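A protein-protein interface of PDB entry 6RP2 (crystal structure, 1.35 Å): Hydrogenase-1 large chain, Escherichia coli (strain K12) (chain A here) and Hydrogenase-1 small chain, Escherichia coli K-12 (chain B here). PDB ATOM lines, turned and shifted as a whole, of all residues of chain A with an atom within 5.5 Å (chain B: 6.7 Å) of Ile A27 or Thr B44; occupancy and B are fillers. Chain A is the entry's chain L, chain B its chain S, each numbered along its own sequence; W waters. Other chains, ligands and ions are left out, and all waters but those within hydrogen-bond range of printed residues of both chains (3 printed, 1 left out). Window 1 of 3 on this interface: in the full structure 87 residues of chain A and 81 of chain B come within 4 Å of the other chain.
The backbone NH (N) of Arg A26 sits at hydrogen-bond distance from the backbone carbonyl oxygen (O) of Asp B43 (2.8 Å). O of Met B46 lies within hydrogen-bond range of NE of Arg A26, at 2.9 Å. O of His B10 sits close to NE2 of His A30, at 3.1 Å. The side-chain hydroxyl (OG1) of Thr B15 lies within hydrogen-bond range of the side-chain carboxylate (OE2) of Glu A28.
O of Thr A25 is in hydrogen-bond range of NE2 of His A571, at 2.7 Å. OE1 of Glu B13 lies close to OG1 of Thr B15. The backbone NH of Glu A28 sits at hydrogen-bond distance from the backbone carbonyl oxygen of Pro A575, at 3.3 Å. The side-chain carboxylate (OD1) of Asp B42 sits close to the backbone NH (N) of Thr B44 (3.4 Å). The backbone carbonyl oxygen (O) of Arg A26 lies close to a ring nitrogen (NE2) of His A571 (3.3 Å). NE2 of His B10 lies close to OG1 of Thr B44, at 3.3 Å.
Among the printed residues, pairs that only touch across the chains: Leu A126 with Thr B44 (3.2 Å), Arg A26 with Thr B44 (3.3 Å), Thr A25 with Asp B43 (3.3 Å), Arg A26 with Leu B45 (3.6 Å), Thr A25 with Met B46 (3.7 Å), Gly A29 with Glu B13 (3.7 Å) and Ile A27 with Thr B44 (3.96 Å).
Of the printed residues of chain B, Arg A26 touches Asp B43 (2.8 Å), Thr B44 (3.3 Å), Leu B45 (3.6 Å) and Met B46 (2.9 Å). Printed residues of chain B within 4 Å of Glu A28: Thr B15. His A571 touches none of the printed residues of chain B. Of the printed residues of chain A, Thr B15 touches Glu A28. Thr B44 touches just these residues of chain A: Arg A26 (3.3 Å), Ile A27 (3.96 Å) and Leu A126 (3.2 Å). Printed residues of chain A within 4 Å of Leu B45: Arg A26 (3.6 Å).
Of the 12 printed residues of chain B, 7 touch a printed residue of chain A. Of the 13 printed residues of chain A, 7 touch a printed residue of chain B. Hydrophobic or aromatic side chains of chain A within 4 Å of the printed part of chain B: His A30 and Leu A126. Among the printed residues, 11 pairs touch across the chains.
Water W2 lies within hydrogen-bond range of the side-chain carboxylate of Glu B13 (2.7 Å), the side-chain hydroxyl of Thr B15 (2.9 Å), the backbone NH of Gly A29 (2.9 Å) and the side-chain hydroxyl of Thr B44 (3.5 Å). Water W1 lies within hydrogen-bond range of the backbone carbonyl oxygen of Gln A125 and the backbone carbonyl oxygen of Leu B45. Water W3 bridges the backbone carbonyl oxygen (O) of Gly A29 (3.1 Å) and the side-chain carboxylate (OE1) of Glu B13 (3.2 Å).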
ATOM      1  N   ILE A  24      -6.734  22.605 -33.676  1.00  0.00           N
ATOM      2  CA  ILE A  24      -7.548  23.083 -32.536  1.00  0.00           C
ATOM      3  C   ILE A  24      -7.162  24.549 -32.333  1.00  0.00           C
ATOM      4  O   ILE A  24      -5.983  24.850 -32.215  1.00  0.00           O
ATOM      5  CB  ILE A  24      -7.303  22.229 -31.275  1.00  0.00           C
ATOM      6  CG1 ILE A  24      -7.623  20.732 -31.474  1.00  0.00           C
ATOM      7  CG2 ILE A  24      -8.030  22.832 -30.086  1.00  0.00           C
ATOM      8  CD1 ILE A  24      -9.090  20.433 -31.637  1.00  0.00           C
ATOM      9  N   THR A  25      -8.121  25.424 -32.270  1.00  0.00           N
ATOM     10  CA  THR A  25      -7.904  26.876 -32.106  1.00  0.00           C
ATOM     11  C   THR A  25      -8.370  27.249 -30.707  1.00  0.00           C
ATOM     12  O   THR A  25      -8.972  26.400 -29.983  1.00  0.00           O
ATOM     13  CB  THR A  25      -8.624  27.634 -33.210  1.00  0.00           C
ATOM     14  OG1 THR A  25      -9.987  27.255 -33.193  1.00  0.00           O
ATOM     15  CG2 THR A  25      -8.007  27.353 -34.554  1.00  0.00           C
ATOM     16  N   ARG A  26      -8.105  28.492 -30.344  1.00  0.00           N
ATOM     17  CA  ARG A  26      -8.446  29.017 -28.992  1.00  0.00           C
ATOM     18  C   ARG A  26      -7.830  28.156 -27.902  1.00  0.00           C
ATOM     19  O   ARG A  26      -8.460  27.885 -26.866  1.00  0.00           O
ATOM     20  CB  ARG A  26      -9.936  29.297 -28.829  1.00  0.00           C
ATOM     21  CG  ARG A  26     -10.299  30.652 -29.432  1.00  0.00           C
ATOM     22  CD  ARG A  26     -11.737  31.040 -29.355  1.00  0.00           C
ATOM     23  NE  ARG A  26     -12.607  30.092 -30.073  1.00  0.00           N
ATOM     24  CZ  ARG A  26     -13.588  29.340 -29.541  1.00  0.00           C
ATOM     25  NH1 ARG A  26     -13.877  29.327 -28.254  1.00  0.00           N
ATOM     26  NH2 ARG A  26     -14.369  28.643 -30.363  1.00  0.00           N
ATOM     27  N   ILE A  27      -6.629  27.715 -28.183  1.00  0.00           N
ATOM     28  CA  ILE A  27      -5.717  27.088 -27.201  1.00  0.00           C
ATOM     29  C   ILE A  27      -4.412  27.829 -27.383  1.00  0.00           C
ATOM     30  O   ILE A  27      -4.184  28.517 -28.417  1.00  0.00           O
ATOM     31  CB  ILE A  27      -5.559  25.575 -27.470  1.00  0.00           C
ATOM     32  CG1 ILE A  27      -4.970  25.292 -28.852  1.00  0.00           C
ATOM     33  CG2 ILE A  27      -6.861  24.862 -27.249  1.00  0.00           C
ATOM     34  CD1 ILE A  27      -4.503  23.895 -29.092  1.00  0.00           C
ATOM     35  N   GLU A  28      -3.444  27.543 -26.515  1.00  0.00           N
ATOM     36  CA  GLU A  28      -2.042  27.879 -26.831  1.00  0.00           C
ATOM     37  C   GLU A  28      -1.450  26.740 -27.683  1.00  0.00           C
ATOM     38  O   GLU A  28      -1.592  25.544 -27.328  1.00  0.00           O
ATOM     39  CB  GLU A  28      -1.228  28.094 -25.544  1.00  0.00           C
ATOM     40  CG  GLU A  28       0.145  28.631 -25.803  1.00  0.00           C
ATOM     41  CD  GLU A  28       1.133  27.702 -26.441  1.00  0.00           C
ATOM     42  OE1 GLU A  28       0.972  26.486 -26.214  1.00  0.00           O
ATOM     43  OE2 GLU A  28       1.992  28.123 -27.235  1.00  0.00           O
ATOM     44  N   GLY A  29      -0.729  27.083 -28.747  1.00  0.00           N
ATOM     45  CA  GLY A  29       0.087  26.139 -29.514  1.00  0.00           C
ATOM     46  C   GLY A  29      -0.723  25.190 -30.363  1.00  0.00           C
ATOM     47  O   GLY A  29      -1.849  25.499 -30.753  1.00  0.00           O
ATOM     48  N   HIS A  30      -0.105  24.078 -30.668  1.00  0.00           N
ATOM     49  CA  HIS A  30      -0.500  23.163 -31.765  1.00  0.00           C
ATOM     50  C   HIS A  30      -1.058  21.850 -31.217  1.00  0.00           C
ATOM     51  O   HIS A  30      -0.317  21.087 -30.630  1.00  0.00           O
ATOM     52  CB  HIS A  30       0.724  22.942 -32.674  1.00  0.00           C
ATOM     53  CG  HIS A  30       1.191  24.204 -33.311  1.00  0.00           C
ATOM     54  ND1 HIS A  30       0.564  24.697 -34.403  1.00  0.00           N
ATOM     55  CD2 HIS A  30       2.214  25.024 -33.029  1.00  0.00           C
ATOM     56  CE1 HIS A  30       1.149  25.839 -34.740  1.00  0.00           C
ATOM     57  NE2 HIS A  30       2.166  26.066 -33.912  1.00  0.00           N
ATOM     58  N   MET A  31      -2.293  21.585 -31.563  1.00  0.00           N
ATOM     59  CA  MET A  31      -2.982  20.323 -31.200  1.00  0.00           C
ATOM     60  C   MET A  31      -3.812  19.841 -32.385  1.00  0.00           C
ATOM     61  O   MET A  31      -4.432  20.640 -33.100  1.00  0.00           O
ATOM     62  CB  MET A  31      -3.905  20.479 -29.986  1.00  0.00           C
ATOM     63  CG  MET A  31      -4.465  19.165 -29.525  1.00  0.00           C
ATOM     64  SD  MET A  31      -5.534  19.385 -28.071  1.00  0.00           S
ATOM     65  CE  MET A  31      -6.149  17.707 -27.968  1.00  0.00           C
ATOM     66  N   GLN A 125     -11.444  34.972 -23.631  1.00  0.00           N
ATOM     67  CA  GLN A 125     -10.882  34.966 -24.985  1.00  0.00           C
ATOM     68  C   GLN A 125     -10.716  33.536 -25.515  1.00  0.00           C
ATOM     69  O   GLN A 125     -10.736  33.378 -26.747  1.00  0.00           O
ATOM     70  CB  GLN A 125      -9.524  35.680 -25.032  1.00  0.00           C
ATOM     71  CG  GLN A 125      -9.652  37.199 -25.135  1.00  0.00           C
ATOM     72  CD  GLN A 125     -10.352  37.858 -23.966  1.00  0.00           C
ATOM     73  OE1 GLN A 125      -9.884  37.727 -22.831  1.00  0.00           O
ATOM     74  NE2 GLN A 125     -11.454  38.569 -24.263  1.00  0.00           N
ATOM     75  N   LEU A 126     -10.532  32.516 -24.680  1.00  0.00           N
ATOM     76  CA  LEU A 126     -10.256  31.152 -25.173  1.00  0.00           C
ATOM     77  C   LEU A 126     -11.536  30.342 -25.132  1.00  0.00           C
ATOM     78  O   LEU A 126     -11.974  29.874 -26.204  1.00  0.00           O
ATOM     79  CB  LEU A 126      -9.079  30.516 -24.454  1.00  0.00           C
ATOM     80  CG  LEU A 126      -7.771  31.306 -24.547  1.00  0.00           C
ATOM     81  CD1 LEU A 126      -6.640  30.655 -23.770  1.00  0.00           C
ATOM     82  CD2 LEU A 126      -7.399  31.550 -25.991  1.00  0.00           C
ATOM     83  N   HIS A 571     -11.473  22.779 -24.491  1.00  0.00           N
ATOM     84  CA  HIS A 571     -11.202  24.121 -23.946  1.00  0.00           C
ATOM     85  C   HIS A 571     -11.407  24.136 -22.428  1.00  0.00           C
ATOM     86  O   HIS A 571     -10.743  24.956 -21.763  1.00  0.00           O
ATOM     87  CB  HIS A 571     -12.081  25.163 -24.631  1.00  0.00           C
ATOM     88  CG  HIS A 571     -11.692  25.456 -26.030  1.00  0.00           C
ATOM     89  ND1 HIS A 571     -12.653  25.862 -26.903  1.00  0.00           N
ATOM     90  CD2 HIS A 571     -10.523  25.449 -26.708  1.00  0.00           C
ATOM     91  CE1 HIS A 571     -12.073  26.074 -28.053  1.00  0.00           C
ATOM     92  NE2 HIS A 571     -10.772  25.886 -27.984  1.00  0.00           N
ATOM     93  N   PRO A 575      -6.073  23.857 -22.668  1.00  0.00           N
ATOM     94  CA  PRO A 575      -4.859  23.226 -23.185  1.00  0.00           C
ATOM     95  C   PRO A 575      -3.774  24.259 -23.496  1.00  0.00           C
ATOM     96  O   PRO A 575      -4.015  25.276 -24.135  1.00  0.00           O
ATOM     97  CB  PRO A 575      -5.303  22.540 -24.486  1.00  0.00           C
ATOM     98  CG  PRO A 575      -6.801  22.404 -24.345  1.00  0.00           C
ATOM     99  CD  PRO A 575      -7.224  23.634 -23.553  1.00  0.00           C
ATOM    100  N   LEU A 577      -0.271  23.693 -25.480  1.00  0.00           N
ATOM    101  CA  LEU A 577       0.449  22.609 -26.156  1.00  0.00           C
ATOM    102  C   LEU A 577       1.947  22.859 -26.128  1.00  0.00           C
ATOM    103  O   LEU A 577       2.722  21.884 -26.148  1.00  0.00           O
ATOM    104  CB  LEU A 577      -0.104  22.440 -27.554  1.00  0.00           C
ATOM    105  CG  LEU A 577      -1.351  21.553 -27.600  1.00  0.00           C
ATOM    106  CD1 LEU A 577      -1.005  20.098 -27.460  1.00  0.00           C
ATOM    107  CD2 LEU A 577      -2.418  21.979 -26.618  1.00  0.00           C
ATOM    108  N   TRP B   8      -2.583  36.026 -39.220  1.00  0.00           N
ATOM    109  CA  TRP B   8      -1.566  35.820 -38.138  1.00  0.00           C
ATOM    110  C   TRP B   8      -1.362  34.322 -37.980  1.00  0.00           C
ATOM    111  O   TRP B   8      -2.296  33.635 -37.569  1.00  0.00           O
ATOM    112  CB  TRP B   8      -1.996  36.564 -36.862  1.00  0.00           C
ATOM    113  CG  TRP B   8      -0.983  36.593 -35.758  1.00  0.00           C
ATOM    114  CD1 TRP B   8      -0.164  35.603 -35.315  1.00  0.00           C
ATOM    115  CD2 TRP B   8      -0.797  37.703 -34.873  1.00  0.00           C
ATOM    116  NE1 TRP B   8       0.543  36.046 -34.203  1.00  0.00           N
ATOM    117  CE2 TRP B   8       0.155  37.318 -33.916  1.00  0.00           C
ATOM    118  CE3 TRP B   8      -1.369  38.984 -34.804  1.00  0.00           C
ATOM    119  CZ2 TRP B   8       0.576  38.188 -32.915  1.00  0.00           C
ATOM    120  CZ3 TRP B   8      -0.977  39.822 -33.778  1.00  0.00           C
ATOM    121  CH2 TRP B   8      -0.012  39.419 -32.849  1.00  0.00           C
ATOM    122  N   HIS B  10       1.201  30.890 -36.698  1.00  0.00           N
ATOM    123  CA  HIS B  10       1.969  30.469 -35.522  1.00  0.00           C
ATOM    124  C   HIS B  10       2.772  29.227 -35.889  1.00  0.00           C
ATOM    125  O   HIS B  10       2.177  28.183 -36.169  1.00  0.00           O
ATOM    126  CB  HIS B  10       0.998  30.140 -34.370  1.00  0.00           C
ATOM    127  CG  HIS B  10       0.184  31.262 -33.880  1.00  0.00           C
ATOM    128  ND1 HIS B  10       0.563  31.943 -32.745  1.00  0.00           N
ATOM    129  CD2 HIS B  10      -0.984  31.774 -34.332  1.00  0.00           C
ATOM    130  CE1 HIS B  10      -0.346  32.899 -32.547  1.00  0.00           C
ATOM    131  NE2 HIS B  10      -1.322  32.821 -33.511  1.00  0.00           N
ATOM    132  N   GLU B  13       6.636  28.109 -31.180  1.00  0.00           N
ATOM    133  CA  GLU B  13       6.449  29.374 -30.415  1.00  0.00           C
ATOM    134  C   GLU B  13       6.122  29.034 -28.982  1.00  0.00           C
ATOM    135  O   GLU B  13       5.791  27.893 -28.671  1.00  0.00           O
ATOM    136  CB  GLU B  13       5.245  30.122 -31.026  1.00  0.00           C
ATOM    137  CG  GLU B  13       3.963  29.390 -30.677  1.00  0.00           C
ATOM    138  CD  GLU B  13       2.637  29.889 -31.152  1.00  0.00           C
ATOM    139  OE1 GLU B  13       1.654  29.056 -31.209  1.00  0.00           O
ATOM    140  OE2 GLU B  13       2.566  31.085 -31.401  1.00  0.00           O
ATOM    141  N   THR B  15       3.929  31.642 -27.653  1.00  0.00           N
ATOM    142  CA  THR B  15       2.747  32.534 -27.706  1.00  0.00           C
ATOM    143  C   THR B  15       2.968  33.817 -26.898  1.00  0.00           C
ATOM    144  O   THR B  15       2.029  34.571 -26.684  1.00  0.00           O
ATOM    145  CB  THR B  15       1.476  31.766 -27.323  1.00  0.00           C
ATOM    146  OG1 THR B  15       1.530  30.506 -28.035  1.00  0.00           O
ATOM    147  CG2 THR B  15       0.223  32.498 -27.743  1.00  0.00           C
ATOM    148  N   THR B  18       1.826  36.986 -29.091  1.00  0.00           N
ATOM    149  CA  THR B  18       0.347  37.235 -29.052  1.00  0.00           C
ATOM    150  C   THR B  18      -0.011  37.856 -27.706  1.00  0.00           C
ATOM    151  O   THR B  18      -0.798  38.787 -27.619  1.00  0.00           O
ATOM    152  CB  THR B  18      -0.428  35.920 -29.273  1.00  0.00           C
ATOM    153  OG1 THR B  18      -0.421  35.629 -30.679  1.00  0.00           O
ATOM    154  CG2 THR B  18      -1.856  35.964 -28.794  1.00  0.00           C
ATOM    155  N   GLU B  19       0.526  37.288 -26.631  1.00  0.00           N
ATOM    156  CA  GLU B  19       0.235  37.809 -25.282  1.00  0.00           C
ATOM    157  C   GLU B  19       0.702  39.255 -25.159  1.00  0.00           C
ATOM    158  O   GLU B  19      -0.014  40.088 -24.623  1.00  0.00           O
ATOM    159  CB  GLU B  19       0.844  36.887 -24.228  1.00  0.00           C
ATOM    160  CG  GLU B  19       0.059  35.580 -24.059  1.00  0.00           C
ATOM    161  CD  GLU B  19      -1.219  35.666 -23.260  1.00  0.00           C
ATOM    162  OE1 GLU B  19      -1.600  36.723 -22.783  1.00  0.00           O
ATOM    163  OE2 GLU B  19      -1.845  34.556 -23.146  1.00  0.00           O
ATOM    164  N   ASP B  42      -6.290  33.742 -36.970  1.00  0.00           N
ATOM    165  CA  ASP B  42      -5.387  33.770 -35.792  1.00  0.00           C
ATOM    166  C   ASP B  42      -5.753  32.587 -34.903  1.00  0.00           C
ATOM    167  O   ASP B  42      -6.768  32.642 -34.212  1.00  0.00           O
ATOM    168  CB  ASP B  42      -5.461  35.112 -35.041  1.00  0.00           C
ATOM    169  CG  ASP B  42      -4.380  35.332 -33.990  1.00  0.00           C
ATOM    170  OD1 ASP B  42      -3.776  34.287 -33.599  1.00  0.00           O
ATOM    171  OD2 ASP B  42      -4.226  36.460 -33.582  1.00  0.00           O
ATOM    172  N   ASP B  43      -4.961  31.528 -34.913  1.00  0.00           N
ATOM    173  CA  ASP B  43      -5.404  30.290 -34.224  1.00  0.00           C
ATOM    174  C   ASP B  43      -5.654  30.590 -32.723  1.00  0.00           C
ATOM    175  O   ASP B  43      -6.571  29.932 -32.173  1.00  0.00           O
ATOM    176  CB  ASP B  43      -4.481  29.096 -34.515  1.00  0.00           C
ATOM    177  CG  ASP B  43      -4.645  28.396 -35.864  1.00  0.00           C
ATOM    178  OD1 ASP B  43      -5.623  28.673 -36.581  1.00  0.00           O
ATOM    179  OD2 ASP B  43      -3.837  27.519 -36.158  1.00  0.00           O
ATOM    180  N   THR B  44      -4.951  31.479 -32.069  1.00  0.00           N
ATOM    181  CA  THR B  44      -5.111  31.684 -30.609  1.00  0.00           C
ATOM    182  C   THR B  44      -6.497  32.231 -30.281  1.00  0.00           C
ATOM    183  O   THR B  44      -7.033  31.938 -29.177  1.00  0.00           O
ATOM    184  CB  THR B  44      -4.068  32.646 -30.024  1.00  0.00           C
ATOM    185  OG1 THR B  44      -2.846  32.297 -30.639  1.00  0.00           O
ATOM    186  CG2 THR B  44      -3.979  32.482 -28.525  1.00  0.00           C
ATOM    187  N   LEU B  45      -7.090  33.041 -31.168  1.00  0.00           N
ATOM    188  CA  LEU B  45      -8.261  33.872 -30.813  1.00  0.00           C
ATOM    189  C   LEU B  45      -9.511  33.556 -31.624  1.00  0.00           C
ATOM    190  O   LEU B  45     -10.595  33.965 -31.201  1.00  0.00           O
ATOM    191  CB  LEU B  45      -7.961  35.365 -30.967  1.00  0.00           C
ATOM    192  CG  LEU B  45      -6.859  35.919 -30.066  1.00  0.00           C
ATOM    193  CD1 LEU B  45      -6.566  37.376 -30.376  1.00  0.00           C
ATOM    194  CD2 LEU B  45      -7.241  35.770 -28.593  1.00  0.00           C
ATOM    195  N   MET B  46      -9.411  32.835 -32.713  1.00  0.00           N
ATOM    196  CA  MET B  46     -10.529  32.726 -33.667  1.00  0.00           C
ATOM    197  C   MET B  46     -11.571  31.683 -33.239  1.00  0.00           C
ATOM    198  O   MET B  46     -11.267  30.684 -32.570  1.00  0.00           O
ATOM    199  CB  MET B  46     -10.004  32.395 -35.070  1.00  0.00           C
ATOM    200  CG  MET B  46      -9.341  31.031 -35.211  1.00  0.00           C
ATOM    201  SD  MET B  46      -8.409  30.894 -36.788  1.00  0.00           S
ATOM    202  CE  MET B  46      -9.761  30.852 -37.946  1.00  0.00           C
ATOM    203  N   GLU B  73       4.267  34.616 -35.984  1.00  0.00           N
ATOM    204  CA  GLU B  73       4.779  34.334 -34.634  1.00  0.00           C
ATOM    205  C   GLU B  73       5.403  32.950 -34.683  1.00  0.00           C
ATOM    206  O   GLU B  73       4.851  32.016 -35.310  1.00  0.00           O
ATOM    207  CB  GLU B  73       3.630  34.429 -33.639  1.00  0.00           C
ATOM    208  CG  GLU B  73       3.966  34.197 -32.159  1.00  0.00           C
ATOM    209  CD  GLU B  73       2.810  34.592 -31.250  1.00  0.00           C
ATOM    210  OE1 GLU B  73       3.002  34.586 -30.034  1.00  0.00           O
ATOM    211  OE2 GLU B  73       1.771  35.000 -31.772  1.00  0.00           O
HETATM  212  O   HOH W   1     -11.051  35.218 -28.736  1.00  0.00           O
HETATM  213  O   HOH W   2      -0.550  29.773 -29.894  1.00  0.00           O
HETATM  214  O   HOH W   3      -0.917  27.784 -32.646  1.00  0.00           O
